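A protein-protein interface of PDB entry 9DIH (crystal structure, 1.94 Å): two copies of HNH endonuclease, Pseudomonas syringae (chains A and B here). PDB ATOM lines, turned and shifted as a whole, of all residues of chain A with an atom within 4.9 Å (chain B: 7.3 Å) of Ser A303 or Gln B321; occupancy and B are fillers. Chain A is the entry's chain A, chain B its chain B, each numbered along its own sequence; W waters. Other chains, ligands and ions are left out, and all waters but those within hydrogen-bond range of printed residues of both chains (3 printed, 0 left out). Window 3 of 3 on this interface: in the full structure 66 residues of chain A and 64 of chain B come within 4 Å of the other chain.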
ATOM      1  N   ILE A 276      -6.137 -25.803 -15.283  1.00  0.00           N
ATOM      2  CA  ILE A 276      -4.869 -25.764 -16.005  1.00  0.00           C
ATOM      3  C   ILE A 276      -4.307 -24.363 -15.985  1.00  0.00           C
ATOM      4  O   ILE A 276      -3.127 -24.146 -15.654  1.00  0.00           O
ATOM      5  CB  ILE A 276      -5.018 -26.256 -17.463  1.00  0.00           C
ATOM      6  CG1 ILE A 276      -5.711 -27.627 -17.574  1.00  0.00           C
ATOM      7  CG2 ILE A 276      -3.646 -26.219 -18.199  1.00  0.00           C
ATOM      8  CD1 ILE A 276      -4.966 -28.790 -16.945  1.00  0.00           C
ATOM      9  N   SER A 277      -5.125 -23.396 -16.383  1.00  0.00           N
ATOM     10  CA  SER A 277      -4.799 -21.990 -16.223  1.00  0.00           C
ATOM     11  C   SER A 277      -4.818 -21.565 -14.764  1.00  0.00           C
ATOM     12  O   SER A 277      -4.030 -20.714 -14.345  1.00  0.00           O
ATOM     13  CB  SER A 277      -5.826 -21.144 -16.968  1.00  0.00           C
ATOM     14  OG  SER A 277      -5.848 -21.419 -18.336  1.00  0.00           O
ATOM     15  N   ALA A 278      -5.711 -22.145 -13.991  1.00  0.00           N
ATOM     16  CA  ALA A 278      -6.011 -21.729 -12.634  1.00  0.00           C
ATOM     17  C   ALA A 278      -6.732 -22.902 -12.009  1.00  0.00           C
ATOM     18  O   ALA A 278      -7.123 -23.848 -12.696  1.00  0.00           O
ATOM     19  CB  ALA A 278      -6.861 -20.480 -12.605  1.00  0.00           C
ATOM     20  N   ILE A 299      -2.765 -29.572 -13.579  1.00  0.00           N
ATOM     21  CA  ILE A 299      -1.315 -29.682 -13.580  1.00  0.00           C
ATOM     22  C   ILE A 299      -0.865 -29.283 -12.175  1.00  0.00           C
ATOM     23  O   ILE A 299      -1.653 -28.728 -11.422  1.00  0.00           O
ATOM     24  CB  ILE A 299      -0.685 -28.778 -14.644  1.00  0.00           C
ATOM     25  CG1 ILE A 299      -1.104 -27.365 -14.347  1.00  0.00           C
ATOM     26  CG2 ILE A 299      -1.053 -29.287 -15.997  1.00  0.00           C
ATOM     27  CD1 ILE A 299      -0.483 -26.284 -15.232  1.00  0.00           C
ATOM     28  N   GLU A 301       1.011 -26.903 -10.926  1.00  0.00           N
ATOM     29  CA  GLU A 301       1.042 -25.481 -10.639  1.00  0.00           C
ATOM     30  C   GLU A 301       0.248 -24.762 -11.713  1.00  0.00           C
ATOM     31  O   GLU A 301       0.815 -24.261 -12.685  1.00  0.00           O
ATOM     32  CB  GLU A 301       2.484 -24.962 -10.571  1.00  0.00           C
ATOM     33  CG  GLU A 301       2.593 -23.539 -10.015  1.00  0.00           C
ATOM     34  CD  GLU A 301       4.037 -23.126  -9.616  1.00  0.00           C
ATOM     35  OE1 GLU A 301       4.880 -22.904 -10.542  1.00  0.00           O
ATOM     36  OE2 GLU A 301       4.309 -23.015  -8.391  1.00  0.00           O
ATOM     37  N   PRO A 302      -1.069 -24.659 -11.555  1.00  0.00           N
ATOM     38  CA  PRO A 302      -1.878 -24.001 -12.583  1.00  0.00           C
ATOM     39  C   PRO A 302      -1.364 -22.592 -12.840  1.00  0.00           C
ATOM     40  O   PRO A 302      -1.066 -21.864 -11.901  1.00  0.00           O
ATOM     41  CB  PRO A 302      -3.299 -24.004 -11.977  1.00  0.00           C
ATOM     42  CG  PRO A 302      -3.298 -25.233 -11.098  1.00  0.00           C
ATOM     43  CD  PRO A 302      -1.899 -25.288 -10.511  1.00  0.00           C
ATOM     44  N   SER A 303      -1.339 -22.202 -14.104  1.00  0.00           N
ATOM     45  CA  SER A 303      -0.733 -20.950 -14.518  1.00  0.00           C
ATOM     46  C   SER A 303      -1.217 -20.556 -15.918  1.00  0.00           C
ATOM     47  O   SER A 303      -1.257 -21.397 -16.836  1.00  0.00           O
ATOM     48  CB  SER A 303       0.799 -21.131 -14.515  1.00  0.00           C
ATOM     49  OG  SER A 303       1.408 -19.997 -15.178  1.00  0.00           O
ATOM     50  N   TYR A 304      -1.553 -19.268 -16.081  1.00  0.00           N
ATOM     51  CA  TYR A 304      -1.818 -18.710 -17.379  1.00  0.00           C
ATOM     52  C   TYR A 304      -0.662 -18.869 -18.345  1.00  0.00           C
ATOM     53  O   TYR A 304      -0.866 -18.747 -19.565  1.00  0.00           O
ATOM     54  CB  TYR A 304      -2.164 -17.214 -17.276  1.00  0.00           C
ATOM     55  CG  TYR A 304      -3.462 -16.784 -16.609  1.00  0.00           C
ATOM     56  CD1 TYR A 304      -4.349 -17.705 -16.103  1.00  0.00           C
ATOM     57  CD2 TYR A 304      -3.781 -15.463 -16.476  1.00  0.00           C
ATOM     58  CE1 TYR A 304      -5.539 -17.289 -15.512  1.00  0.00           C
ATOM     59  CE2 TYR A 304      -4.976 -15.064 -15.864  1.00  0.00           C
ATOM     60  CZ  TYR A 304      -5.850 -16.018 -15.388  1.00  0.00           C
ATOM     61  OH  TYR A 304      -7.025 -15.677 -14.739  1.00  0.00           O
ATOM     62  N   ALA A 305       0.554 -19.089 -17.846  1.00  0.00           N
ATOM     63  CA  ALA A 305       1.730 -19.031 -18.717  1.00  0.00           C
ATOM     64  C   ALA A 305       2.170 -20.353 -19.233  1.00  0.00           C
ATOM     65  O   ALA A 305       3.258 -20.458 -19.818  1.00  0.00           O
ATOM     66  CB  ALA A 305       2.890 -18.411 -17.967  1.00  0.00           C
ATOM     67  N   MET A 306       1.362 -21.446 -19.022  1.00  0.00           N
ATOM     68  CA  MET A 306       1.945 -22.746 -19.133  1.00  0.00           C
ATOM     69  C   MET A 306       2.118 -23.292 -20.552  1.00  0.00           C
ATOM     70  O   MET A 306       2.747 -24.343 -20.708  1.00  0.00           O
ATOM     71  CB  MET A 306       1.109 -23.736 -18.283  1.00  0.00           C
ATOM     72  CG  MET A 306      -0.392 -23.899 -18.652  1.00  0.00           C
ATOM     73  SD  MET A 306      -0.680 -24.961 -20.133  1.00  0.00           S
ATOM     74  CE  MET A 306      -0.055 -26.540 -19.555  1.00  0.00           C
ATOM     75  N   LEU B 297       3.807 -11.867  -0.920  1.00  0.00           N
ATOM     76  CA  LEU B 297       4.708 -12.094  -2.032  1.00  0.00           C
ATOM     77  C   LEU B 297       5.815 -11.066  -1.928  1.00  0.00           C
ATOM     78  O   LEU B 297       5.537  -9.880  -1.874  1.00  0.00           O
ATOM     79  CB  LEU B 297       3.968 -11.920  -3.360  1.00  0.00           C
ATOM     80  CG  LEU B 297       4.784 -12.504  -4.494  1.00  0.00           C
ATOM     81  CD1 LEU B 297       4.822 -14.033  -4.460  1.00  0.00           C
ATOM     82  CD2 LEU B 297       4.218 -12.058  -5.799  1.00  0.00           C
ATOM     83  N   ALA B 315       7.746 -11.608 -15.266  1.00  0.00           N
ATOM     84  CA  ALA B 315       7.962 -12.636 -14.249  1.00  0.00           C
ATOM     85  C   ALA B 315       7.150 -12.380 -12.974  1.00  0.00           C
ATOM     86  O   ALA B 315       6.743 -13.337 -12.288  1.00  0.00           O
ATOM     87  CB  ALA B 315       9.443 -12.732 -13.898  1.00  0.00           C
ATOM     88  N   PHE B 316       6.964 -11.119 -12.615  1.00  0.00           N
ATOM     89  CA  PHE B 316       6.141 -10.799 -11.478  1.00  0.00           C
ATOM     90  C   PHE B 316       4.712 -11.232 -11.724  1.00  0.00           C
ATOM     91  O   PHE B 316       4.084 -11.815 -10.848  1.00  0.00           O
ATOM     92  CB  PHE B 316       6.198  -9.287 -11.220  1.00  0.00           C
ATOM     93  CG  PHE B 316       5.094  -8.726 -10.325  1.00  0.00           C
ATOM     94  CD1 PHE B 316       5.166  -8.903  -8.969  1.00  0.00           C
ATOM     95  CD2 PHE B 316       4.050  -8.082 -10.827  1.00  0.00           C
ATOM     96  CE1 PHE B 316       4.158  -8.421  -8.179  1.00  0.00           C
ATOM     97  CE2 PHE B 316       3.064  -7.616 -10.049  1.00  0.00           C
ATOM     98  CZ  PHE B 316       3.132  -7.774  -8.743  1.00  0.00           C
ATOM     99  N   ARG B 317       4.186 -10.945 -12.913  1.00  0.00           N
ATOM    100  CA  ARG B 317       2.830 -11.296 -13.213  1.00  0.00           C
ATOM    101  C   ARG B 317       2.623 -12.802 -13.190  1.00  0.00           C
ATOM    102  O   ARG B 317       1.522 -13.265 -12.851  1.00  0.00           O
ATOM    103  CB  ARG B 317       2.493 -10.732 -14.597  1.00  0.00           C
ATOM    104  CG  ARG B 317       1.056 -10.964 -15.088  1.00  0.00           C
ATOM    105  CD  ARG B 317       0.945 -12.221 -15.924  1.00  0.00           C
ATOM    106  NE  ARG B 317       1.952 -12.301 -16.950  1.00  0.00           N
ATOM    107  CZ  ARG B 317       2.129 -11.455 -17.950  1.00  0.00           C
ATOM    108  NH1 ARG B 317       1.272 -10.521 -18.205  1.00  0.00           N
ATOM    109  NH2 ARG B 317       3.189 -11.598 -18.757  1.00  0.00           N
ATOM    110  N   ASP B 318       3.634 -13.580 -13.584  1.00  0.00           N
ATOM    111  CA  ASP B 318       3.477 -15.022 -13.667  1.00  0.00           C
ATOM    112  C   ASP B 318       3.472 -15.627 -12.296  1.00  0.00           C
ATOM    113  O   ASP B 318       2.641 -16.486 -11.995  1.00  0.00           O
ATOM    114  CB  ASP B 318       4.613 -15.640 -14.465  1.00  0.00           C
ATOM    115  CG  ASP B 318       4.512 -15.334 -15.952  1.00  0.00           C
ATOM    116  OD1 ASP B 318       3.470 -14.745 -16.361  1.00  0.00           O
ATOM    117  OD2 ASP B 318       5.444 -15.726 -16.690  1.00  0.00           O
ATOM    118  N   ALA B 319       4.322 -15.115 -11.412  1.00  0.00           N
ATOM    119  CA  ALA B 319       4.298 -15.562 -10.035  1.00  0.00           C
ATOM    120  C   ALA B 319       3.078 -15.046  -9.318  1.00  0.00           C
ATOM    121  O   ALA B 319       2.455 -15.770  -8.561  1.00  0.00           O
ATOM    122  CB  ALA B 319       5.556 -15.081  -9.319  1.00  0.00           C
ATOM    123  N   LEU B 320       2.710 -13.788  -9.533  1.00  0.00           N
ATOM    124  CA  LEU B 320       1.508 -13.288  -8.907  1.00  0.00           C
ATOM    125  C   LEU B 320       0.298 -14.137  -9.268  1.00  0.00           C
ATOM    126  O   LEU B 320      -0.503 -14.491  -8.397  1.00  0.00           O
ATOM    127  CB  LEU B 320       1.290 -11.845  -9.308  1.00  0.00           C
ATOM    128  CG  LEU B 320      -0.006 -11.177  -8.863  1.00  0.00           C
ATOM    129  CD1 LEU B 320      -0.003 -11.088  -7.375  1.00  0.00           C
ATOM    130  CD2 LEU B 320      -0.077  -9.789  -9.462  1.00  0.00           C
ATOM    131  N   GLN B 321       0.107 -14.430 -10.547  1.00  0.00           N
ATOM    132  CA  GLN B 321      -1.124 -15.137 -10.937  1.00  0.00           C
ATOM    133  C   GLN B 321      -1.159 -16.558 -10.351  1.00  0.00           C
ATOM    134  O   GLN B 321      -2.220 -17.070  -9.978  1.00  0.00           O
ATOM    135  CB  GLN B 321      -1.262 -15.187 -12.425  1.00  0.00           C
ATOM    136  CG  GLN B 321      -2.556 -15.881 -12.943  1.00  0.00           C
ATOM    137  CD  GLN B 321      -2.403 -17.378 -13.092  1.00  0.00           C
ATOM    138  OE1 GLN B 321      -1.345 -17.889 -13.481  1.00  0.00           O
ATOM    139  NE2 GLN B 321      -3.460 -18.123 -12.737  1.00  0.00           N
ATOM    140  N   ILE B 322      -0.022 -17.214 -10.269  1.00  0.00           N
ATOM    141  CA  ILE B 322       0.009 -18.533  -9.679  1.00  0.00           C
ATOM    142  C   ILE B 322      -0.477 -18.474  -8.236  1.00  0.00           C
ATOM    143  O   ILE B 322      -1.095 -19.427  -7.748  1.00  0.00           O
ATOM    144  CB  ILE B 322       1.425 -19.115  -9.756  1.00  0.00           C
ATOM    145  CG1 ILE B 322       1.659 -19.729 -11.131  1.00  0.00           C
ATOM    146  CG2 ILE B 322       1.660 -20.147  -8.608  1.00  0.00           C
ATOM    147  CD1 ILE B 322       3.144 -19.843 -11.439  1.00  0.00           C
ATOM    148  N   ARG B 323      -0.120 -17.415  -7.499  1.00  0.00           N
ATOM    149  CA  ARG B 323      -0.477 -17.334  -6.103  1.00  0.00           C
ATOM    150  C   ARG B 323      -1.917 -16.841  -5.942  1.00  0.00           C
ATOM    151  O   ARG B 323      -2.571 -17.186  -4.957  1.00  0.00           O
ATOM    152  CB  ARG B 323       0.447 -16.386  -5.347  1.00  0.00           C
ATOM    153  CG  ARG B 323       1.909 -16.785  -5.573  1.00  0.00           C
ATOM    154  CD  ARG B 323       2.100 -18.219  -4.983  1.00  0.00           C
ATOM    155  NE  ARG B 323       3.497 -18.598  -4.992  1.00  0.00           N
ATOM    156  CZ  ARG B 323       3.943 -19.731  -4.526  1.00  0.00           C
ATOM    157  NH1 ARG B 323       3.114 -20.620  -4.017  1.00  0.00           N
ATOM    158  NH2 ARG B 323       5.255 -19.949  -4.517  1.00  0.00           N
ATOM    159  N   LEU B 324      -2.405 -16.044  -6.874  1.00  0.00           N
ATOM    160  CA  LEU B 324      -3.782 -15.596  -6.768  1.00  0.00           C
ATOM    161  C   LEU B 324      -4.740 -16.760  -6.936  1.00  0.00           C
ATOM    162  O   LEU B 324      -5.779 -16.805  -6.270  1.00  0.00           O
ATOM    163  CB  LEU B 324      -4.079 -14.521  -7.800  1.00  0.00           C
ATOM    164  CG  LEU B 324      -3.361 -13.200  -7.545  1.00  0.00           C
ATOM    165  CD1 LEU B 324      -3.867 -12.182  -8.549  1.00  0.00           C
ATOM    166  CD2 LEU B 324      -3.554 -12.621  -6.134  1.00  0.00           C
ATOM    167  N   SER B 325      -4.438 -17.675  -7.860  1.00  0.00           N
ATOM    168  CA  SER B 325      -5.225 -18.887  -8.032  1.00  0.00           C
ATOM    169  C   SER B 325      -5.274 -19.679  -6.750  1.00  0.00           C
ATOM    170  O   SER B 325      -6.350 -20.154  -6.346  1.00  0.00           O
ATOM    171  CB  SER B 325      -4.682 -19.722  -9.161  1.00  0.00           C
ATOM    172  OG  SER B 325      -5.084 -21.099  -9.193  1.00  0.00           O
ATOM    173  N   GLN B 326      -4.137 -19.805  -6.060  1.00  0.00           N
ATOM    174  CA  GLN B 326      -4.114 -20.558  -4.809  1.00  0.00           C
ATOM    175  C   GLN B 326      -4.935 -19.854  -3.731  1.00  0.00           C
ATOM    176  O   GLN B 326      -5.634 -20.492  -2.954  1.00  0.00           O
ATOM    177  CB  GLN B 326      -2.669 -20.734  -4.352  1.00  0.00           C
ATOM    178  CG  GLN B 326      -1.817 -21.453  -5.333  1.00  0.00           C
ATOM    179  CD  GLN B 326      -0.338 -21.562  -4.913  1.00  0.00           C
ATOM    180  OE1 GLN B 326       0.069 -21.089  -3.843  1.00  0.00           O
ATOM    181  NE2 GLN B 326       0.471 -22.168  -5.774  1.00  0.00           N
ATOM    182  N   LEU B 327      -4.827 -18.546  -3.630  1.00  0.00           N
ATOM    183  CA  LEU B 327      -5.556 -17.821  -2.627  1.00  0.00           C
ATOM    184  C   LEU B 327      -7.060 -17.872  -2.901  1.00  0.00           C
ATOM    185  O   LEU B 327      -7.848 -18.101  -1.998  1.00  0.00           O
ATOM    186  CB  LEU B 327      -5.084 -16.360  -2.596  1.00  0.00           C
ATOM    187  CG  LEU B 327      -3.712 -16.196  -1.942  1.00  0.00           C
ATOM    188  CD1 LEU B 327      -3.330 -14.755  -2.014  1.00  0.00           C
ATOM    189  CD2 LEU B 327      -3.675 -16.619  -0.491  1.00  0.00           C
ATOM    190  N   GLU B 328      -7.484 -17.633  -4.137  1.00  0.00           N
ATOM    191  CA  GLU B 328      -8.904 -17.646  -4.429  1.00  0.00           C
ATOM    192  C   GLU B 328      -9.508 -19.036  -4.226  1.00  0.00           C
ATOM    193  O   GLU B 328     -10.693 -19.165  -3.888  1.00  0.00           O
ATOM    194  CB  GLU B 328      -9.150 -17.174  -5.860  1.00  0.00           C
ATOM    195  CG  GLU B 328      -8.776 -15.730  -6.061  1.00  0.00           C
ATOM    196  CD  GLU B 328      -9.049 -15.308  -7.486  1.00  0.00           C
ATOM    197  OE1 GLU B 328      -9.777 -16.079  -8.171  1.00  0.00           O
ATOM    198  OE2 GLU B 328      -8.549 -14.238  -7.921  1.00  0.00           O
ATOM    199  N   LEU B 352      -3.725  -7.945 -15.568  1.00  0.00           N
ATOM    200  CA  LEU B 352      -3.955  -9.359 -15.341  1.00  0.00           C
ATOM    201  C   LEU B 352      -5.420  -9.661 -15.002  1.00  0.00           C
ATOM    202  O   LEU B 352      -5.920 -10.769 -15.290  1.00  0.00           O
ATOM    203  CB  LEU B 352      -3.039  -9.837 -14.187  1.00  0.00           C
ATOM    204  CG  LEU B 352      -3.251 -11.270 -13.693  1.00  0.00           C
ATOM    205  CD1 LEU B 352      -2.838 -12.251 -14.719  1.00  0.00           C
ATOM    206  CD2 LEU B 352      -2.483 -11.557 -12.422  1.00  0.00           C
ATOM    207  N   TYR B 361     -11.336  -7.897  -5.355  1.00  0.00           N
ATOM    208  CA  TYR B 361     -10.078  -7.372  -4.824  1.00  0.00           C
ATOM    209  C   TYR B 361     -10.330  -5.977  -4.295  1.00  0.00           C
ATOM    210  O   TYR B 361     -10.946  -5.158  -4.982  1.00  0.00           O
ATOM    211  CB  TYR B 361      -9.006  -7.361  -5.954  1.00  0.00           C
ATOM    212  CG  TYR B 361      -8.396  -8.740  -6.178  1.00  0.00           C
ATOM    213  CD1 TYR B 361      -7.367  -9.174  -5.411  1.00  0.00           C
ATOM    214  CD2 TYR B 361      -8.871  -9.587  -7.172  1.00  0.00           C
ATOM    215  CE1 TYR B 361      -6.835 -10.457  -5.580  1.00  0.00           C
ATOM    216  CE2 TYR B 361      -8.369 -10.849  -7.308  1.00  0.00           C
ATOM    217  CZ  TYR B 361      -7.361 -11.282  -6.522  1.00  0.00           C
ATOM    218  OH  TYR B 361      -6.866 -12.551  -6.665  1.00  0.00           O
HETATM  219  O   HOH W   1       1.072 -17.325 -14.011  1.00  0.00           O
HETATM  220  O   HOH W   2      -1.415 -21.757  -9.214  1.00  0.00           O
HETATM  221  O   HOH W   3      -7.203 -12.819 -14.136  1.00  0.00           O
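Of the 10 printed residues of chain A, 7 touch a printed residue of chain B. Printed residues of chain A that touch a printed residue of chain B: Ser A277, Ala A278, Glu A301, Pro A302, Ser A303, Tyr A304 and Ala A305. Among the printed residues, 9 pairs touch across the chains.
Of the printed residues of chain B, Ala A278 touches Ser B325. Printed residues of chain B within 4 Å of Glu A301: Ile B322. Of the printed residues of chain B, Ser A303 touches Gln B321 and Ile B322. Of the printed residues of chain B, Tyr A304 touches Gln B321 and Leu B352. Met A306 touches none of the printed residues of chain B. Leu B297 touches none of the printed residues of chain A. Of chain A, only Ser A277, Ser A303 and Tyr A304 come within 4 Å of Gln B321. Of the printed residues of chain A, Leu B352 touches Tyr A304 (3.7 Å). The nearest residue of chain B that does not touch Ser A303 is Asp B318 (4.9 Å). The nearest residue of chain A that does not touch Gln B321 is Ala A278 (4.1 Å).
N of Ser A303 lies within hydrogen-bond range of O of Ile A276 (3.1 Å). O of Ser A277 lies within hydrogen-bond range of N of Ser A303, 3.1 Å away. The backbone NH (N) of Tyr A304 is in hydrogen-bond range of the backbone carbonyl oxygen (O) of Ser A277. The side-chain carboxylate (OD1) of Asp B318 is in salt-bridge range of the guanidinium group (NE) of Arg B317 (2.9 Å). The side-chain hydroxyl (OG) of Ser A303 is in hydrogen-bond range of the backbone NH (N) of Ala A305, at 2.9 Å.
Water W1 lies within hydrogen-bond range of OE1 of Gln B321 (2.5 Å), O of Asp B318 (2.7 Å) and OG of Ser A303 (2.9 Å). Water W3 bridges O of Leu B352 (2.7 Å) and OH of Tyr A304 (2.9 Å). Water W2 lies within hydrogen-bond range of the backbone carbonyl oxygen (O) of Pro A302 (2.7 Å) and the backbone carbonyl oxygen (O) of Ile B322 (2.8 Å).
No position is printed for both chains.
The backbone carbonyl oxygen (O) of Ser A277 is in hydrogen-bond range of the side-chain amide nitrogen (NE2) of Gln B321 (3.1 Å). The side-chain amide oxygen (OE1) of Gln B321 lies within hydrogen-bond range of the backbone NH (N) of Tyr A304 (3.0 Å).
Ser B325 touches Ala A278. Ile B322 touches Glu A301 (CD1 to OE1, 3.6 Å). Pro A302 touches Ile B322 (O to CG1, 3.5 Å). Gln B321 touches Ser A303 (OE1 to CA, 3.3 Å). Ile B322 touches Ser A303. CE2 of Tyr A304 touches CD1 of Leu B352, 3.7 Å away. CB of Ala A305 touches OD2 of Asp B318, at 3.9 Å.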
